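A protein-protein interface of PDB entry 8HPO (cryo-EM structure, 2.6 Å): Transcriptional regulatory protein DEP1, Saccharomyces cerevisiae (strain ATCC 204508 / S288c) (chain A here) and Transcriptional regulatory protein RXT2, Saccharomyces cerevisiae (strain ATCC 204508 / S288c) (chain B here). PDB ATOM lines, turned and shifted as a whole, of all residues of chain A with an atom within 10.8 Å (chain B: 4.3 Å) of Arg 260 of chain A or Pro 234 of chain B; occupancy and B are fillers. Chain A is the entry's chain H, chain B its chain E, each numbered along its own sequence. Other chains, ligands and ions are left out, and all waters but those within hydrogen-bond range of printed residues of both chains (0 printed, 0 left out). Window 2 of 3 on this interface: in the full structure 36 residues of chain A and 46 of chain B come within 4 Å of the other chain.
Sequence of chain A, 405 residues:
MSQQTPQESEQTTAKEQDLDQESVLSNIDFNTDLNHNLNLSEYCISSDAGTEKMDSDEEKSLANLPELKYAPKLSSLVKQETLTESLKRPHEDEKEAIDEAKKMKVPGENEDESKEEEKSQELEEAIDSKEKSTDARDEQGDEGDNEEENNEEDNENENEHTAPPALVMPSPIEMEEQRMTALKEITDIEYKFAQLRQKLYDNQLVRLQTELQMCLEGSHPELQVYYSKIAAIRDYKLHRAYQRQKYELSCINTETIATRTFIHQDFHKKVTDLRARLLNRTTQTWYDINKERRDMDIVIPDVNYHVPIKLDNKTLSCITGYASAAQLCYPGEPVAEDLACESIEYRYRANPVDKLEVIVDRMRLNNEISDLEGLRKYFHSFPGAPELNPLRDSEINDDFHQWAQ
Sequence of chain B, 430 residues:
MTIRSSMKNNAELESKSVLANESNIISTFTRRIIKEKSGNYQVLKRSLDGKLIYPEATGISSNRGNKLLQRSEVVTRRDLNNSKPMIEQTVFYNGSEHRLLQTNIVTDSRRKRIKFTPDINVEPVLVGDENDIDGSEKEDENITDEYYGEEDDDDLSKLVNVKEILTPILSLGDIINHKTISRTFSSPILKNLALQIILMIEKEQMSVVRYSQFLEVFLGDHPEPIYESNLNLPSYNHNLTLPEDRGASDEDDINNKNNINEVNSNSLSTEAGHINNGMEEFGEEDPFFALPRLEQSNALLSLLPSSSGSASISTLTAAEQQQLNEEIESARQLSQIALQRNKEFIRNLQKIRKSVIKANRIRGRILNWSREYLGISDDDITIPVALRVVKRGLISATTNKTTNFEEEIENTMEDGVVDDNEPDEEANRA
The guanidinium group (NH1) of Arg 260 of chain A sits at hydrogen-bond distance from the backbone carbonyl oxygen (O) of Pro 234 of chain B (3.3 Å).
NE of Arg 260 of chain A sits at hydrogen-bond distance from O of Phe 288 of chain B (3.1 Å).
O of Pro 287 of chain B is in hydrogen-bond range of NH1 of Arg 260 of chain A (2.7 Å).
The side-chain hydroxyl (OG1) of Thr 256 of chain A is in hydrogen-bond range of the side-chain hydroxyl (OH) of Tyr 236 of chain B, 3.3 Å away.
O of Arg 260 of chain A sits at hydrogen-bond distance from ND1 of His 264 of chain A.
O of Asn 253 of chain A lies within hydrogen-bond range of OG1 of Thr 256 of chain A (2.9 Å).
The side-chain hydroxyl (OG1) of Thr 256 of chain A sits close to the backbone carbonyl oxygen (O) of Ile 252 of chain A, 3.4 Å away.
O of Ile 257 of chain A lies within hydrogen-bond range of OG1 of Thr 261 of chain A (3.4 Å).
Tyr 236 of chain B touches Ile 257 of chain A (OH to CG1, 3.6 Å).
Arg 260 of chain A touches Leu 233 of chain B.
O of Ala 290 of chain B touches NE2 of His 264 of chain A (3.5 Å).
Printed residues of chain B within 4 Å of Thr 256 of chain A: Tyr 236.
Of the printed residues of chain B, Ile 257 of chain A touches Tyr 236 (3.6 Å).
Printed residues of chain B within 4 Å of His 264 of chain A: Ala 290.
Leu 233 of chain B touches just one residue of chain A: Arg 260 (3.7 Å).
No residue of chain A comes within 4 Å of Ser 235 of chain B.
Of chain A, only Thr 256 and Ile 257 come within 4 Å of Tyr 236 of chain B.
Of the printed residues of chain A, Pro 287 of chain B touches Arg 260 (2.7 Å).
Ala 290 of chain B touches just one residue of chain A: His 264.
The nearest printed residue of chain B that does not touch Arg 260 of chain A is Tyr 236 of chain B (4.4 Å).
The nearest residue of chain A that does not touch Pro 234 of chain B is His 264 of chain A (7.8 Å).
The nearest printed residue of chain B that does not touch Thr 256 of chain A is Phe 288 of chain B (5.6 Å).
Printed residues of chain A that touch a printed residue of chain B: Thr 256, Ile 257, Arg 260 and His 264.
Hydrophobic or aromatic side chains of chain A that line the printed part of chain B: Ile 257 and His 264.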
ATOM      1  N   ILE A 252      -4.393 -19.882  17.631  1.00  0.00           N
ATOM      2  CA  ILE A 252      -4.637 -18.530  18.134  1.00  0.00           C
ATOM      3  C   ILE A 252      -3.400 -17.657  17.961  1.00  0.00           C
ATOM      4  O   ILE A 252      -3.492 -16.485  17.561  1.00  0.00           O
ATOM      5  CB  ILE A 252      -5.084 -18.594  19.602  1.00  0.00           C
ATOM      6  CG1 ILE A 252      -6.423 -19.307  19.707  1.00  0.00           C
ATOM      7  CG2 ILE A 252      -5.176 -17.209  20.189  1.00  0.00           C
ATOM      8  CD1 ILE A 252      -6.949 -19.387  21.100  1.00  0.00           C
ATOM      9  N   ASN A 253      -2.225 -18.215  18.252  1.00  0.00           N
ATOM     10  CA  ASN A 253      -0.975 -17.489  18.053  1.00  0.00           C
ATOM     11  C   ASN A 253      -0.862 -16.917  16.640  1.00  0.00           C
ATOM     12  O   ASN A 253      -0.711 -15.703  16.451  1.00  0.00           O
ATOM     13  CB  ASN A 253       0.196 -18.425  18.349  1.00  0.00           C
ATOM     14  CG  ASN A 253       1.479 -17.690  18.604  1.00  0.00           C
ATOM     15  OD1 ASN A 253       1.554 -16.844  19.488  1.00  0.00           O
ATOM     16  ND2 ASN A 253       2.508 -18.015  17.838  1.00  0.00           N
ATOM     17  N   THR A 254      -0.915 -17.792  15.631  1.00  0.00           N
ATOM     18  CA  THR A 254      -0.658 -17.357  14.262  1.00  0.00           C
ATOM     19  C   THR A 254      -1.741 -16.421  13.754  1.00  0.00           C
ATOM     20  O   THR A 254      -1.453 -15.513  12.964  1.00  0.00           O
ATOM     21  CB  THR A 254      -0.538 -18.562  13.336  1.00  0.00           C
ATOM     22  OG1 THR A 254      -1.640 -19.443  13.560  1.00  0.00           O
ATOM     23  CG2 THR A 254       0.745 -19.303  13.596  1.00  0.00           C
ATOM     24  N   GLU A 255      -2.980 -16.595  14.216  1.00  0.00           N
ATOM     25  CA  GLU A 255      -4.028 -15.677  13.790  1.00  0.00           C
ATOM     26  C   GLU A 255      -3.789 -14.275  14.334  1.00  0.00           C
ATOM     27  O   GLU A 255      -3.963 -13.283  13.610  1.00  0.00           O
ATOM     28  CB  GLU A 255      -5.392 -16.201  14.214  1.00  0.00           C
ATOM     29  CG  GLU A 255      -5.915 -17.293  13.316  1.00  0.00           C
ATOM     30  CD  GLU A 255      -7.385 -17.567  13.535  1.00  0.00           C
ATOM     31  OE1 GLU A 255      -7.893 -17.240  14.624  1.00  0.00           O
ATOM     32  OE2 GLU A 255      -8.032 -18.113  12.621  1.00  0.00           O
ATOM     33  N   THR A 256      -3.354 -14.160  15.594  1.00  0.00           N
ATOM     34  CA  THR A 256      -3.114 -12.817  16.118  1.00  0.00           C
ATOM     35  C   THR A 256      -1.890 -12.179  15.474  1.00  0.00           C
ATOM     36  O   THR A 256      -1.873 -10.966  15.231  1.00  0.00           O
ATOM     37  CB  THR A 256      -2.987 -12.835  17.639  1.00  0.00           C
ATOM     38  OG1 THR A 256      -1.846 -13.602  18.020  1.00  0.00           O
ATOM     39  CG2 THR A 256      -4.242 -13.415  18.267  1.00  0.00           C
ATOM     40  N   ILE A 257      -0.880 -12.976  15.132  1.00  0.00           N
ATOM     41  CA  ILE A 257       0.269 -12.415  14.422  1.00  0.00           C
ATOM     42  C   ILE A 257      -0.155 -11.862  13.064  1.00  0.00           C
ATOM     43  O   ILE A 257       0.226 -10.747  12.668  1.00  0.00           O
ATOM     44  CB  ILE A 257       1.376 -13.471  14.283  1.00  0.00           C
ATOM     45  CG1 ILE A 257       2.013 -13.736  15.639  1.00  0.00           C
ATOM     46  CG2 ILE A 257       2.419 -13.019  13.293  1.00  0.00           C
ATOM     47  CD1 ILE A 257       3.023 -14.829  15.615  1.00  0.00           C
ATOM     48  N   ALA A 258      -0.972 -12.626  12.337  1.00  0.00           N
ATOM     49  CA  ALA A 258      -1.405 -12.189  11.016  1.00  0.00           C
ATOM     50  C   ALA A 258      -2.218 -10.905  11.096  1.00  0.00           C
ATOM     51  O   ALA A 258      -2.010  -9.976  10.307  1.00  0.00           O
ATOM     52  CB  ALA A 258      -2.205 -13.295  10.337  1.00  0.00           C
ATOM     53  N   THR A 259      -3.151 -10.824  12.042  1.00  0.00           N
ATOM     54  CA  THR A 259      -3.968  -9.614  12.090  1.00  0.00           C
ATOM     55  C   THR A 259      -3.182  -8.403  12.602  1.00  0.00           C
ATOM     56  O   THR A 259      -3.513  -7.266  12.253  1.00  0.00           O
ATOM     57  CB  THR A 259      -5.218  -9.866  12.919  1.00  0.00           C
ATOM     58  OG1 THR A 259      -5.984  -8.663  13.027  1.00  0.00           O
ATOM     59  CG2 THR A 259      -4.841 -10.321  14.263  1.00  0.00           C
ATOM     60  N   ARG A 260      -2.131  -8.616  13.401  1.00  0.00           N
ATOM     61  CA  ARG A 260      -1.180  -7.545  13.701  1.00  0.00           C
ATOM     62  C   ARG A 260      -0.586  -6.964  12.419  1.00  0.00           C
ATOM     63  O   ARG A 260      -0.588  -5.737  12.201  1.00  0.00           O
ATOM     64  CB  ARG A 260      -0.080  -8.109  14.598  1.00  0.00           C
ATOM     65  CG  ARG A 260       0.706  -7.150  15.464  1.00  0.00           C
ATOM     66  CD  ARG A 260       1.458  -7.970  16.511  1.00  0.00           C
ATOM     67  NE  ARG A 260       2.531  -7.255  17.191  1.00  0.00           N
ATOM     68  CZ  ARG A 260       3.821  -7.387  16.902  1.00  0.00           C
ATOM     69  NH1 ARG A 260       4.726  -6.702  17.577  1.00  0.00           N
ATOM     70  NH2 ARG A 260       4.207  -8.190  15.931  1.00  0.00           N
ATOM     71  N   THR A 261      -0.077  -7.842  11.552  1.00  0.00           N
ATOM     72  CA  THR A 261       0.442  -7.378  10.267  1.00  0.00           C
ATOM     73  C   THR A 261      -0.623  -6.632   9.466  1.00  0.00           C
ATOM     74  O   THR A 261      -0.335  -5.613   8.821  1.00  0.00           O
ATOM     75  CB  THR A 261       0.973  -8.556   9.464  1.00  0.00           C
ATOM     76  OG1 THR A 261       2.011  -9.202  10.205  1.00  0.00           O
ATOM     77  CG2 THR A 261       1.527  -8.092   8.133  1.00  0.00           C
ATOM     78  N   PHE A 262      -1.864  -7.118   9.502  1.00  0.00           N
ATOM     79  CA  PHE A 262      -2.924  -6.477   8.731  1.00  0.00           C
ATOM     80  C   PHE A 262      -3.194  -5.067   9.237  1.00  0.00           C
ATOM     81  O   PHE A 262      -3.410  -4.139   8.444  1.00  0.00           O
ATOM     82  CB  PHE A 262      -4.207  -7.312   8.780  1.00  0.00           C
ATOM     83  CG  PHE A 262      -4.060  -8.697   8.216  1.00  0.00           C
ATOM     84  CD1 PHE A 262      -3.020  -9.013   7.366  1.00  0.00           C
ATOM     85  CD2 PHE A 262      -4.966  -9.686   8.542  1.00  0.00           C
ATOM     86  CE1 PHE A 262      -2.884 -10.278   6.865  1.00  0.00           C
ATOM     87  CE2 PHE A 262      -4.832 -10.950   8.033  1.00  0.00           C
ATOM     88  CZ  PHE A 262      -3.794 -11.245   7.198  1.00  0.00           C
ATOM     89  N   ILE A 263      -3.183  -4.887  10.558  1.00  0.00           N
ATOM     90  CA  ILE A 263      -3.438  -3.574  11.147  1.00  0.00           C
ATOM     91  C   ILE A 263      -2.390  -2.575  10.681  1.00  0.00           C
ATOM     92  O   ILE A 263      -2.707  -1.444  10.271  1.00  0.00           O
ATOM     93  CB  ILE A 263      -3.473  -3.686  12.680  1.00  0.00           C
ATOM     94  CG1 ILE A 263      -4.878  -4.035  13.154  1.00  0.00           C
ATOM     95  CG2 ILE A 263      -3.004  -2.410  13.324  1.00  0.00           C
ATOM     96  CD1 ILE A 263      -4.921  -4.724  14.481  1.00  0.00           C
ATOM     97  N   HIS A 264      -1.128  -2.994  10.680  1.00  0.00           N
ATOM     98  CA  HIS A 264      -0.093  -2.034  10.309  1.00  0.00           C
ATOM     99  C   HIS A 264      -0.111  -1.726   8.810  1.00  0.00           C
ATOM    100  O   HIS A 264       0.108  -0.572   8.403  1.00  0.00           O
ATOM    101  CB  HIS A 264       1.267  -2.533  10.777  1.00  0.00           C
ATOM    102  CG  HIS A 264       1.527  -2.245  12.222  1.00  0.00           C
ATOM    103  ND1 HIS A 264       0.892  -2.920  13.240  1.00  0.00           N
ATOM    104  CD2 HIS A 264       2.305  -1.315  12.820  1.00  0.00           C
ATOM    105  CE1 HIS A 264       1.290  -2.438  14.402  1.00  0.00           C
ATOM    106  NE2 HIS A 264       2.147  -1.462  14.173  1.00  0.00           N
ATOM    107  N   GLN A 265      -0.422  -2.721   7.974  1.00  0.00           N
ATOM    108  CA  GLN A 265      -0.504  -2.457   6.538  1.00  0.00           C
ATOM    109  C   GLN A 265      -1.649  -1.500   6.207  1.00  0.00           C
ATOM    110  O   GLN A 265      -1.499  -0.600   5.364  1.00  0.00           O
ATOM    111  CB  GLN A 265      -0.658  -3.768   5.767  1.00  0.00           C
ATOM    112  CG  GLN A 265       0.649  -4.514   5.540  1.00  0.00           C
ATOM    113  CD  GLN A 265       0.484  -5.774   4.709  1.00  0.00           C
ATOM    114  OE1 GLN A 265      -0.424  -6.573   4.935  1.00  0.00           O
ATOM    115  NE2 GLN A 265       1.373  -5.960   3.751  1.00  0.00           N
ATOM    116  N   ASP A 266      -2.801  -1.674   6.857  1.00  0.00           N
ATOM    117  CA  ASP A 266      -3.917  -0.773   6.598  1.00  0.00           C
ATOM    118  C   ASP A 266      -3.588   0.659   7.017  1.00  0.00           C
ATOM    119  O   ASP A 266      -3.947   1.617   6.312  1.00  0.00           O
ATOM    120  CB  ASP A 266      -5.171  -1.270   7.311  1.00  0.00           C
ATOM    121  CG  ASP A 266      -6.440  -1.029   6.507  1.00  0.00           C
ATOM    122  OD1 ASP A 266      -7.538  -1.020   7.104  1.00  0.00           O
ATOM    123  OD2 ASP A 266      -6.344  -0.845   5.278  1.00  0.00           O
ATOM    124  N   PHE A 267      -2.900   0.831   8.152  1.00  0.00           N
ATOM    125  CA  PHE A 267      -2.490   2.182   8.541  1.00  0.00           C
ATOM    126  C   PHE A 267      -1.601   2.823   7.480  1.00  0.00           C
ATOM    127  O   PHE A 267      -1.792   3.993   7.114  1.00  0.00           O
ATOM    128  CB  PHE A 267      -1.775   2.164   9.892  1.00  0.00           C
ATOM    129  CG  PHE A 267      -1.229   3.503  10.304  1.00  0.00           C
ATOM    130  CD1 PHE A 267       0.090   3.832  10.060  1.00  0.00           C
ATOM    131  CD2 PHE A 267      -2.029   4.426  10.933  1.00  0.00           C
ATOM    132  CE1 PHE A 267       0.587   5.056  10.430  1.00  0.00           C
ATOM    133  CE2 PHE A 267      -1.532   5.643  11.300  1.00  0.00           C
ATOM    134  CZ  PHE A 267      -0.225   5.955  11.056  1.00  0.00           C
ATOM    135  N   HIS A 268      -0.604   2.079   6.995  1.00  0.00           N
ATOM    136  CA  HIS A 268       0.309   2.638   5.998  1.00  0.00           C
ATOM    137  C   HIS A 268      -0.436   3.087   4.747  1.00  0.00           C
ATOM    138  O   HIS A 268      -0.178   4.180   4.204  1.00  0.00           O
ATOM    139  CB  HIS A 268       1.368   1.605   5.647  1.00  0.00           C
ATOM    140  CG  HIS A 268       2.389   2.087   4.672  1.00  0.00           C
ATOM    141  ND1 HIS A 268       2.435   1.650   3.369  1.00  0.00           N
ATOM    142  CD2 HIS A 268       3.422   2.950   4.817  1.00  0.00           C
ATOM    143  CE1 HIS A 268       3.445   2.229   2.748  1.00  0.00           C
ATOM    144  NE2 HIS A 268       4.059   3.024   3.604  1.00  0.00           N
ATOM    145  N   ASN B 232       9.826  -4.768  10.410  1.00  0.00           N
ATOM    146  CA  ASN B 232      10.647  -5.570  11.302  1.00  0.00           C
ATOM    147  C   ASN B 232      10.100  -5.431  12.709  1.00  0.00           C
ATOM    148  O   ASN B 232      10.799  -4.971  13.616  1.00  0.00           O
ATOM    149  CB  ASN B 232      12.109  -5.134  11.248  1.00  0.00           C
ATOM    150  CG  ASN B 232      12.701  -5.247   9.865  1.00  0.00           C
ATOM    151  OD1 ASN B 232      13.206  -4.273   9.313  1.00  0.00           O
ATOM    152  ND2 ASN B 232      12.652  -6.441   9.299  1.00  0.00           N
ATOM    153  N   LEU B 233       8.845  -5.821  12.888  1.00  0.00           N
ATOM    154  CA  LEU B 233       8.207  -5.702  14.182  1.00  0.00           C
ATOM    155  C   LEU B 233       8.974  -6.538  15.200  1.00  0.00           C
ATOM    156  O   LEU B 233       9.529  -7.587  14.852  1.00  0.00           O
ATOM    157  CB  LEU B 233       6.751  -6.161  14.097  1.00  0.00           C
ATOM    158  CG  LEU B 233       5.718  -5.128  13.641  1.00  0.00           C
ATOM    159  CD1 LEU B 233       4.503  -5.806  13.062  1.00  0.00           C
ATOM    160  CD2 LEU B 233       5.306  -4.240  14.786  1.00  0.00           C
ATOM    161  N   PRO B 234       9.051  -6.101  16.452  1.00  0.00           N
ATOM    162  CA  PRO B 234       9.740  -6.903  17.462  1.00  0.00           C
ATOM    163  C   PRO B 234       8.868  -8.059  17.910  1.00  0.00           C
ATOM    164  O   PRO B 234       7.696  -7.887  18.249  1.00  0.00           O
ATOM    165  CB  PRO B 234       9.970  -5.905  18.599  1.00  0.00           C
ATOM    166  CG  PRO B 234       8.829  -4.982  18.483  1.00  0.00           C
ATOM    167  CD  PRO B 234       8.558  -4.831  17.010  1.00  0.00           C
ATOM    168  N   SER B 235       9.455  -9.250  17.906  1.00  0.00           N
ATOM    169  CA  SER B 235       8.709 -10.440  18.276  1.00  0.00           C
ATOM    170  C   SER B 235       8.428 -10.448  19.770  1.00  0.00           C
ATOM    171  O   SER B 235       9.234  -9.995  20.584  1.00  0.00           O
ATOM    172  CB  SER B 235       9.477 -11.697  17.886  1.00  0.00           C
ATOM    173  OG  SER B 235       8.879 -12.841  18.462  1.00  0.00           O
ATOM    174  N   TYR B 236       7.268 -10.979  20.126  1.00  0.00           N
ATOM    175  CA  TYR B 236       6.824 -11.055  21.504  1.00  0.00           C
ATOM    176  C   TYR B 236       6.680 -12.515  21.904  1.00  0.00           C
ATOM    177  O   TYR B 236       7.016 -13.426  21.146  1.00  0.00           O
ATOM    178  CB  TYR B 236       5.505 -10.302  21.704  1.00  0.00           C
ATOM    179  CG  TYR B 236       4.331 -10.836  20.917  1.00  0.00           C
ATOM    180  CD1 TYR B 236       4.347 -10.872  19.529  1.00  0.00           C
ATOM    181  CD2 TYR B 236       3.198 -11.287  21.563  1.00  0.00           C
ATOM    182  CE1 TYR B 236       3.274 -11.356  18.815  1.00  0.00           C
ATOM    183  CE2 TYR B 236       2.121 -11.771  20.859  1.00  0.00           C
ATOM    184  CZ  TYR B 236       2.162 -11.801  19.485  1.00  0.00           C
ATOM    185  OH  TYR B 236       1.086 -12.285  18.782  1.00  0.00           O
ATOM    186  N   PRO B 287       6.570  -5.332  23.453  1.00  0.00           N
ATOM    187  CA  PRO B 287       6.899  -5.501  22.036  1.00  0.00           C
ATOM    188  C   PRO B 287       5.704  -5.921  21.201  1.00  0.00           C
ATOM    189  O   PRO B 287       5.821  -6.009  19.975  1.00  0.00           O
ATOM    190  CB  PRO B 287       7.976  -6.589  22.054  1.00  0.00           C
ATOM    191  CG  PRO B 287       7.739  -7.339  23.291  1.00  0.00           C
ATOM    192  CD  PRO B 287       7.054  -6.453  24.275  1.00  0.00           C
ATOM    193  N   PHE B 288       4.570  -6.191  21.848  1.00  0.00           N
ATOM    194  CA  PHE B 288       3.307  -6.335  21.138  1.00  0.00           C
ATOM    195  C   PHE B 288       2.887  -5.026  20.493  1.00  0.00           C
ATOM    196  O   PHE B 288       2.581  -4.996  19.296  1.00  0.00           O
ATOM    197  CB  PHE B 288       2.228  -6.816  22.108  1.00  0.00           C
ATOM    198  CG  PHE B 288       0.911  -7.125  21.458  1.00  0.00           C
ATOM    199  CD1 PHE B 288      -0.212  -6.382  21.757  1.00  0.00           C
ATOM    200  CD2 PHE B 288       0.787  -8.176  20.572  1.00  0.00           C
ATOM    201  CE1 PHE B 288      -1.428  -6.665  21.172  1.00  0.00           C
ATOM    202  CE2 PHE B 288      -0.430  -8.460  19.983  1.00  0.00           C
ATOM    203  CZ  PHE B 288      -1.537  -7.701  20.289  1.00  0.00           C
ATOM    204  N   ALA B 290       4.479  -2.391  19.644  1.00  0.00           N
ATOM    205  CA  ALA B 290       5.523  -1.594  19.023  1.00  0.00           C
ATOM    206  C   ALA B 290       5.225  -1.362  17.544  1.00  0.00           C
ATOM    207  O   ALA B 290       4.264  -1.890  16.984  1.00  0.00           O
ATOM    208  CB  ALA B 290       6.881  -2.262  19.191  1.00  0.00           C
ATOM    209  N   ARG B 293       9.255  -0.085  12.405  1.00  0.00           N
ATOM    210  CA  ARG B 293      10.683   0.106  12.138  1.00  0.00           C
ATOM    211  C   ARG B 293      11.008  -0.205  10.677  1.00  0.00           C
ATOM    212  O   ARG B 293      11.803  -1.092  10.368  1.00  0.00           O
ATOM    213  CB  ARG B 293      11.558  -0.739  13.070  1.00  0.00           C
ATOM    214  CG  ARG B 293      11.067  -0.864  14.495  1.00  0.00           C
ATOM    215  CD  ARG B 293      12.127  -1.498  15.369  1.00  0.00           C
ATOM    216  NE  ARG B 293      12.195  -2.944  15.190  1.00  0.00           N
ATOM    217  CZ  ARG B 293      12.932  -3.753  15.943  1.00  0.00           C
ATOM    218  NH1 ARG B 293      12.933  -5.059  15.717  1.00  0.00           N
ATOM    219  NH2 ARG B 293      13.667  -3.255  16.926  1.00  0.00           N
